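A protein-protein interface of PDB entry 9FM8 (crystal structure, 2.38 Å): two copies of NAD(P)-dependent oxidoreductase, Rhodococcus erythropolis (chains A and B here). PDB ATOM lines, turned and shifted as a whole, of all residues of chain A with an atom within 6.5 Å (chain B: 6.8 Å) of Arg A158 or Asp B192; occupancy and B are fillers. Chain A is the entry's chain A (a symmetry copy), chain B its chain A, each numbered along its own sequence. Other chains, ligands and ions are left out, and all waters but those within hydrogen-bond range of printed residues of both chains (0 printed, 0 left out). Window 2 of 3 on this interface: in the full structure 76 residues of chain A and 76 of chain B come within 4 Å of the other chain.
O of Asp B192 sits at hydrogen-bond distance from NH2 of Arg A158, 3.0 Å away.
O of Tyr B187 sits at hydrogen-bond distance from OG of Ser B190 (2.7 Å). The side-chain carboxylate (OE2) of Glu B191 sits at hydrogen-bond distance from the side-chain hydroxyl (OH) of Tyr B187, at 2.9 Å. The backbone carbonyl oxygen (O) of Val B188 lies within hydrogen-bond range of the backbone NH (N) of Val B193 (3.1 Å). OG of Ser A132 sits close to O of Arg A158. The backbone NH of Ala A161 is in hydrogen-bond range of the side-chain hydroxyl of Ser A132.
Among the printed residues, merely in contact across the chains: Val A164 with Tyr B187 (3.6 Å), Arg A158 with Glu B191 (3.8 Å), Val A164 with Val B188 (3.8 Å), Val A164 with Glu B191 (3.8 Å), Pro A93 with Glu B191 (3.9 Å), Val A164 with Val B193 (3.9 Å) and Ala A161 with Val B193 (3.98 Å).
Of chain B, only Glu B191 and Asp B192 come within 4 Å of Arg A158. Asp B192 touches just one residue of chain A: Arg A158. Of the printed residues of chain B, Pro A93 touches Glu B191 (3.9 Å). Of the printed residues of chain A, Val B188 touches Val A164. Of the printed residues of chain A, Glu B191 touches Pro A93, Arg A158 and Val A164. Of the printed residues of chain B, Val A164 touches Tyr B187 (3.6 Å), Val B188 (3.8 Å), Glu B191 (3.8 Å) and Val B193 (3.9 Å). The nearest printed residue of chain A that does not touch Asp B192 is Val A164 (6.6 Å). The nearest printed residue of chain B that does not touch Ala A161 is Val B188 (6.5 Å).
Printed residues of chain A that touch a printed residue of chain B: Pro A93, Arg A158, Ala A161 and Val A164. Hydrophobic or aromatic side chains of chain A within 4 Å of the printed part of chain B: Pro A93, Ala A161 and Val A164. Of the 8 printed residues of chain B, 5 touch a printed residue of chain A. Printed residues of chain B that touch a printed residue of chain A: Tyr B187, Val B188, Glu B191, Asp B192 and Val B193. Among the printed residues, no Asp or Glu carboxylate lies within 4 Å of a Lys or Arg side-chain nitrogen of the other chain.
No position is printed for both chains. Of the 8 pairs that touch across the chains among the printed residues, none has its exchanged pair printed and touching as well.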
ATOM      1  N   PRO A  93      -2.727  29.603   3.065  1.00  0.00           N
ATOM      2  CA  PRO A  93      -1.803  28.646   3.664  1.00  0.00           C
ATOM      3  C   PRO A  93      -0.674  29.355   4.406  1.00  0.00           C
ATOM      4  O   PRO A  93      -0.263  28.896   5.462  1.00  0.00           O
ATOM      5  CB  PRO A  93      -1.316  27.794   2.468  1.00  0.00           C
ATOM      6  CG  PRO A  93      -1.595  28.661   1.258  1.00  0.00           C
ATOM      7  CD  PRO A  93      -2.839  29.464   1.604  1.00  0.00           C
ATOM      8  N   ASN A  97       0.668  28.857   8.221  1.00  0.00           N
ATOM      9  CA  ASN A  97       1.981  28.287   8.446  1.00  0.00           C
ATOM     10  C   ASN A  97       2.702  29.192   9.443  1.00  0.00           C
ATOM     11  O   ASN A  97       3.330  28.700  10.375  1.00  0.00           O
ATOM     12  CB  ASN A  97       2.695  28.026   7.120  1.00  0.00           C
ATOM     13  CG  ASN A  97       3.921  27.158   7.290  1.00  0.00           C
ATOM     14  OD1 ASN A  97       4.099  26.514   8.331  1.00  0.00           O
ATOM     15  ND2 ASN A  97       4.782  27.125   6.287  1.00  0.00           N
ATOM     16  N   ASP A 112      -4.511  23.092  12.171  1.00  0.00           N
ATOM     17  CA  ASP A 112      -5.263  24.112  11.447  1.00  0.00           C
ATOM     18  C   ASP A 112      -6.500  23.455  10.860  1.00  0.00           C
ATOM     19  O   ASP A 112      -6.443  22.294  10.474  1.00  0.00           O
ATOM     20  CB  ASP A 112      -4.465  24.775  10.342  1.00  0.00           C
ATOM     21  CG  ASP A 112      -5.155  25.961   9.691  1.00  0.00           C
ATOM     22  OD1 ASP A 112      -6.233  25.757   9.107  1.00  0.00           O
ATOM     23  OD2 ASP A 112      -4.613  27.081   9.795  1.00  0.00           O
ATOM     24  N   TYR A 131      -8.806  19.109   8.771  1.00  0.00           N
ATOM     25  CA  TYR A 131      -7.700  19.543   9.607  1.00  0.00           C
ATOM     26  C   TYR A 131      -6.371  19.235   8.926  1.00  0.00           C
ATOM     27  O   TYR A 131      -6.274  18.213   8.248  1.00  0.00           O
ATOM     28  CB  TYR A 131      -7.784  18.762  10.921  1.00  0.00           C
ATOM     29  CG  TYR A 131      -9.092  18.908  11.687  1.00  0.00           C
ATOM     30  CD1 TYR A 131      -9.261  19.919  12.629  1.00  0.00           C
ATOM     31  CD2 TYR A 131     -10.164  18.050  11.461  1.00  0.00           C
ATOM     32  CE1 TYR A 131     -10.445  20.060  13.343  1.00  0.00           C
ATOM     33  CE2 TYR A 131     -11.348  18.178  12.170  1.00  0.00           C
ATOM     34  CZ  TYR A 131     -11.490  19.183  13.121  1.00  0.00           C
ATOM     35  OH  TYR A 131     -12.661  19.322  13.821  1.00  0.00           O
ATOM     36  N   SER A 132      -5.346  20.076   9.139  1.00  0.00           N
ATOM     37  CA  SER A 132      -3.991  19.741   8.711  1.00  0.00           C
ATOM     38  C   SER A 132      -2.944  20.223   9.718  1.00  0.00           C
ATOM     39  O   SER A 132      -3.175  21.171  10.460  1.00  0.00           O
ATOM     40  CB  SER A 132      -3.700  20.270   7.323  1.00  0.00           C
ATOM     41  OG  SER A 132      -4.054  21.635   7.193  1.00  0.00           O
ATOM     42  N   GLY A 133      -1.784  19.555   9.727  1.00  0.00           N
ATOM     43  CA  GLY A 133      -0.694  19.879  10.637  1.00  0.00           C
ATOM     44  C   GLY A 133      -0.126  18.608  11.270  1.00  0.00           C
ATOM     45  O   GLY A 133      -0.280  17.534  10.708  1.00  0.00           O
ATOM     46  N   TYR A 154      -8.274  14.418   8.469  1.00  0.00           N
ATOM     47  CA  TYR A 154      -6.942  14.975   8.476  1.00  0.00           C
ATOM     48  C   TYR A 154      -6.384  14.927   7.061  1.00  0.00           C
ATOM     49  O   TYR A 154      -6.149  13.849   6.533  1.00  0.00           O
ATOM     50  CB  TYR A 154      -6.113  14.148   9.451  1.00  0.00           C
ATOM     51  CG  TYR A 154      -4.646  14.502   9.331  1.00  0.00           C
ATOM     52  CD1 TYR A 154      -4.141  15.672   9.879  1.00  0.00           C
ATOM     53  CD2 TYR A 154      -3.778  13.685   8.631  1.00  0.00           C
ATOM     54  CE1 TYR A 154      -2.805  16.006   9.758  1.00  0.00           C
ATOM     55  CE2 TYR A 154      -2.434  13.995   8.522  1.00  0.00           C
ATOM     56  CZ  TYR A 154      -1.950  15.162   9.076  1.00  0.00           C
ATOM     57  OH  TYR A 154      -0.633  15.446   8.909  1.00  0.00           O
ATOM     58  N   VAL A 155      -6.132  16.100   6.475  1.00  0.00           N
ATOM     59  CA  VAL A 155      -5.850  16.194   5.056  1.00  0.00           C
ATOM     60  C   VAL A 155      -4.392  16.522   4.754  1.00  0.00           C
ATOM     61  O   VAL A 155      -4.108  16.939   3.642  1.00  0.00           O
ATOM     62  CB  VAL A 155      -6.767  17.264   4.443  1.00  0.00           C
ATOM     63  CG1 VAL A 155      -8.233  16.968   4.749  1.00  0.00           C
ATOM     64  CG2 VAL A 155      -6.382  18.675   4.867  1.00  0.00           C
ATOM     65  N   GLY A 156      -3.464  16.362   5.703  1.00  0.00           N
ATOM     66  CA  GLY A 156      -2.047  16.506   5.382  1.00  0.00           C
ATOM     67  C   GLY A 156      -1.244  17.275   6.431  1.00  0.00           C
ATOM     68  O   GLY A 156      -1.790  18.041   7.222  1.00  0.00           O
ATOM     69  N   ALA A 157       0.077  17.073   6.387  1.00  0.00           N
ATOM     70  CA  ALA A 157       0.994  17.562   7.403  1.00  0.00           C
ATOM     71  C   ALA A 157       1.298  19.042   7.194  1.00  0.00           C
ATOM     72  O   ALA A 157       1.728  19.719   8.134  1.00  0.00           O
ATOM     73  CB  ALA A 157       2.259  16.739   7.400  1.00  0.00           C
ATOM     74  N   ARG A 158       1.058  19.546   5.977  1.00  0.00           N
ATOM     75  CA  ARG A 158       1.181  20.974   5.737  1.00  0.00           C
ATOM     76  C   ARG A 158       0.061  21.676   6.504  1.00  0.00           C
ATOM     77  O   ARG A 158      -1.118  21.394   6.292  1.00  0.00           O
ATOM     78  CB  ARG A 158       1.198  21.234   4.229  1.00  0.00           C
ATOM     79  CG  ARG A 158       1.844  22.549   3.812  1.00  0.00           C
ATOM     80  CD  ARG A 158       2.116  22.647   2.301  1.00  0.00           C
ATOM     81  NE  ARG A 158       2.575  21.396   1.674  1.00  0.00           N
ATOM     82  CZ  ARG A 158       3.774  21.126   1.127  1.00  0.00           C
ATOM     83  NH1 ARG A 158       4.792  21.968   1.245  1.00  0.00           N
ATOM     84  NH2 ARG A 158       3.954  19.987   0.469  1.00  0.00           N
ATOM     85  N   PRO A 159       0.383  22.557   7.478  1.00  0.00           N
ATOM     86  CA  PRO A 159      -0.635  23.373   8.156  1.00  0.00           C
ATOM     87  C   PRO A 159      -1.579  24.118   7.215  1.00  0.00           C
ATOM     88  O   PRO A 159      -2.772  24.252   7.489  1.00  0.00           O
ATOM     89  CB  PRO A 159       0.184  24.379   8.990  1.00  0.00           C
ATOM     90  CG  PRO A 159       1.567  23.762   9.127  1.00  0.00           C
ATOM     91  CD  PRO A 159       1.747  22.791   7.981  1.00  0.00           C
ATOM     92  N   GLY A 160      -1.030  24.634   6.110  1.00  0.00           N
ATOM     93  CA  GLY A 160      -1.817  25.437   5.188  1.00  0.00           C
ATOM     94  C   GLY A 160      -2.775  24.612   4.324  1.00  0.00           C
ATOM     95  O   GLY A 160      -3.520  25.183   3.531  1.00  0.00           O
ATOM     96  N   ALA A 161      -2.769  23.280   4.484  1.00  0.00           N
ATOM     97  CA  ALA A 161      -3.420  22.391   3.536  1.00  0.00           C
ATOM     98  C   ALA A 161      -4.947  22.466   3.627  1.00  0.00           C
ATOM     99  O   ALA A 161      -5.632  22.414   2.604  1.00  0.00           O
ATOM    100  CB  ALA A 161      -2.927  20.986   3.751  1.00  0.00           C
ATOM    101  N   ALA A 162      -5.499  22.577   4.837  1.00  0.00           N
ATOM    102  CA  ALA A 162      -6.947  22.636   4.956  1.00  0.00           C
ATOM    103  C   ALA A 162      -7.472  23.939   4.353  1.00  0.00           C
ATOM    104  O   ALA A 162      -8.621  24.006   3.912  1.00  0.00           O
ATOM    105  CB  ALA A 162      -7.381  22.455   6.390  1.00  0.00           C
ATOM    106  N   VAL A 164      -5.955  25.471   1.704  1.00  0.00           N
ATOM    107  CA  VAL A 164      -5.797  25.375   0.266  1.00  0.00           C
ATOM    108  C   VAL A 164      -7.058  24.739  -0.304  1.00  0.00           C
ATOM    109  O   VAL A 164      -7.646  25.229  -1.255  1.00  0.00           O
ATOM    110  CB  VAL A 164      -4.533  24.576  -0.089  1.00  0.00           C
ATOM    111  CG1 VAL A 164      -4.508  24.146  -1.550  1.00  0.00           C
ATOM    112  CG2 VAL A 164      -3.278  25.364   0.253  1.00  0.00           C
ATOM    113  N   TYR B 187      -5.059  24.169  -8.594  1.00  0.00           N
ATOM    114  CA  TYR B 187      -4.570  25.002  -7.507  1.00  0.00           C
ATOM    115  C   TYR B 187      -4.054  24.102  -6.380  1.00  0.00           C
ATOM    116  O   TYR B 187      -2.953  24.323  -5.895  1.00  0.00           O
ATOM    117  CB  TYR B 187      -5.631  25.988  -7.010  1.00  0.00           C
ATOM    118  CG  TYR B 187      -5.230  26.693  -5.721  1.00  0.00           C
ATOM    119  CD1 TYR B 187      -4.014  27.355  -5.621  1.00  0.00           C
ATOM    120  CD2 TYR B 187      -6.038  26.645  -4.587  1.00  0.00           C
ATOM    121  CE1 TYR B 187      -3.628  27.981  -4.444  1.00  0.00           C
ATOM    122  CE2 TYR B 187      -5.659  27.263  -3.401  1.00  0.00           C
ATOM    123  CZ  TYR B 187      -4.448  27.936  -3.325  1.00  0.00           C
ATOM    124  OH  TYR B 187      -4.054  28.561  -2.172  1.00  0.00           O
ATOM    125  N   VAL B 188      -4.831  23.076  -6.002  1.00  0.00           N
ATOM    126  CA  VAL B 188      -4.515  22.224  -4.863  1.00  0.00           C
ATOM    127  C   VAL B 188      -3.203  21.492  -5.129  1.00  0.00           C
ATOM    128  O   VAL B 188      -2.442  21.204  -4.203  1.00  0.00           O
ATOM    129  CB  VAL B 188      -5.628  21.198  -4.552  1.00  0.00           C
ATOM    130  CG1 VAL B 188      -5.219  20.215  -3.459  1.00  0.00           C
ATOM    131  CG2 VAL B 188      -6.948  21.866  -4.199  1.00  0.00           C
ATOM    132  N   ARG B 189      -2.984  21.134  -6.398  1.00  0.00           N
ATOM    133  CA  ARG B 189      -1.811  20.368  -6.773  1.00  0.00           C
ATOM    134  C   ARG B 189      -0.593  21.287  -6.795  1.00  0.00           C
ATOM    135  O   ARG B 189       0.515  20.814  -6.571  1.00  0.00           O
ATOM    136  CB  ARG B 189      -2.048  19.665  -8.114  1.00  0.00           C
ATOM    137  CG  ARG B 189      -1.117  18.483  -8.372  1.00  0.00           C
ATOM    138  CD  ARG B 189      -1.356  17.804  -9.726  1.00  0.00           C
ATOM    139  NE  ARG B 189      -1.235  18.773 -10.827  1.00  0.00           N
ATOM    140  CZ  ARG B 189      -1.447  18.547 -12.122  1.00  0.00           C
ATOM    141  NH1 ARG B 189      -1.685  17.316 -12.548  1.00  0.00           N
ATOM    142  NH2 ARG B 189      -1.403  19.554 -12.986  1.00  0.00           N
ATOM    143  N   SER B 190      -0.824  22.584  -7.051  1.00  0.00           N
ATOM    144  CA  SER B 190       0.234  23.574  -7.178  1.00  0.00           C
ATOM    145  C   SER B 190       0.721  24.045  -5.806  1.00  0.00           C
ATOM    146  O   SER B 190       1.767  24.685  -5.720  1.00  0.00           O
ATOM    147  CB  SER B 190      -0.185  24.761  -8.053  1.00  0.00           C
ATOM    148  OG  SER B 190      -1.167  25.583  -7.437  1.00  0.00           O
ATOM    149  N   GLU B 191      -0.033  23.739  -4.743  1.00  0.00           N
ATOM    150  CA  GLU B 191       0.384  24.059  -3.383  1.00  0.00           C
ATOM    151  C   GLU B 191       0.988  22.800  -2.759  1.00  0.00           C
ATOM    152  O   GLU B 191       1.137  22.722  -1.542  1.00  0.00           O
ATOM    153  CB  GLU B 191      -0.760  24.648  -2.549  1.00  0.00           C
ATOM    154  CG  GLU B 191      -1.300  26.000  -3.033  1.00  0.00           C
ATOM    155  CD  GLU B 191      -0.621  27.278  -2.542  1.00  0.00           C
ATOM    156  OE1 GLU B 191       0.503  27.162  -2.012  1.00  0.00           O
ATOM    157  OE2 GLU B 191      -1.203  28.394  -2.655  1.00  0.00           O
ATOM    158  N   ASP B 192       1.371  21.840  -3.614  1.00  0.00           N
ATOM    159  CA  ASP B 192       1.850  20.522  -3.204  1.00  0.00           C
ATOM    160  C   ASP B 192       0.963  19.974  -2.086  1.00  0.00           C
ATOM    161  O   ASP B 192       1.461  19.370  -1.149  1.00  0.00           O
ATOM    162  CB  ASP B 192       3.342  20.507  -2.883  1.00  0.00           C
ATOM    163  N   VAL B 193      -0.354  20.176  -2.215  1.00  0.00           N
ATOM    164  CA  VAL B 193      -1.341  19.476  -1.404  1.00  0.00           C
ATOM    165  C   VAL B 193      -1.890  18.334  -2.253  1.00  0.00           C
ATOM    166  O   VAL B 193      -2.049  18.486  -3.458  1.00  0.00           O
ATOM    167  CB  VAL B 193      -2.473  20.413  -0.921  1.00  0.00           C
ATOM    168  CG1 VAL B 193      -3.583  19.681  -0.170  1.00  0.00           C
ATOM    169  CG2 VAL B 193      -1.936  21.549  -0.061  1.00  0.00           C
ATOM    170  N   ALA B 194      -2.187  17.201  -1.615  1.00  0.00           N
ATOM    171  CA  ALA B 194      -2.681  16.030  -2.325  1.00  0.00           C
ATOM    172  C   ALA B 194      -4.137  16.207  -2.777  1.00  0.00           C
ATOM    173  O   ALA B 194      -5.065  16.400  -1.987  1.00  0.00           O
ATOM    174  CB  ALA B 194      -2.506  14.804  -1.462  1.00  0.00           C
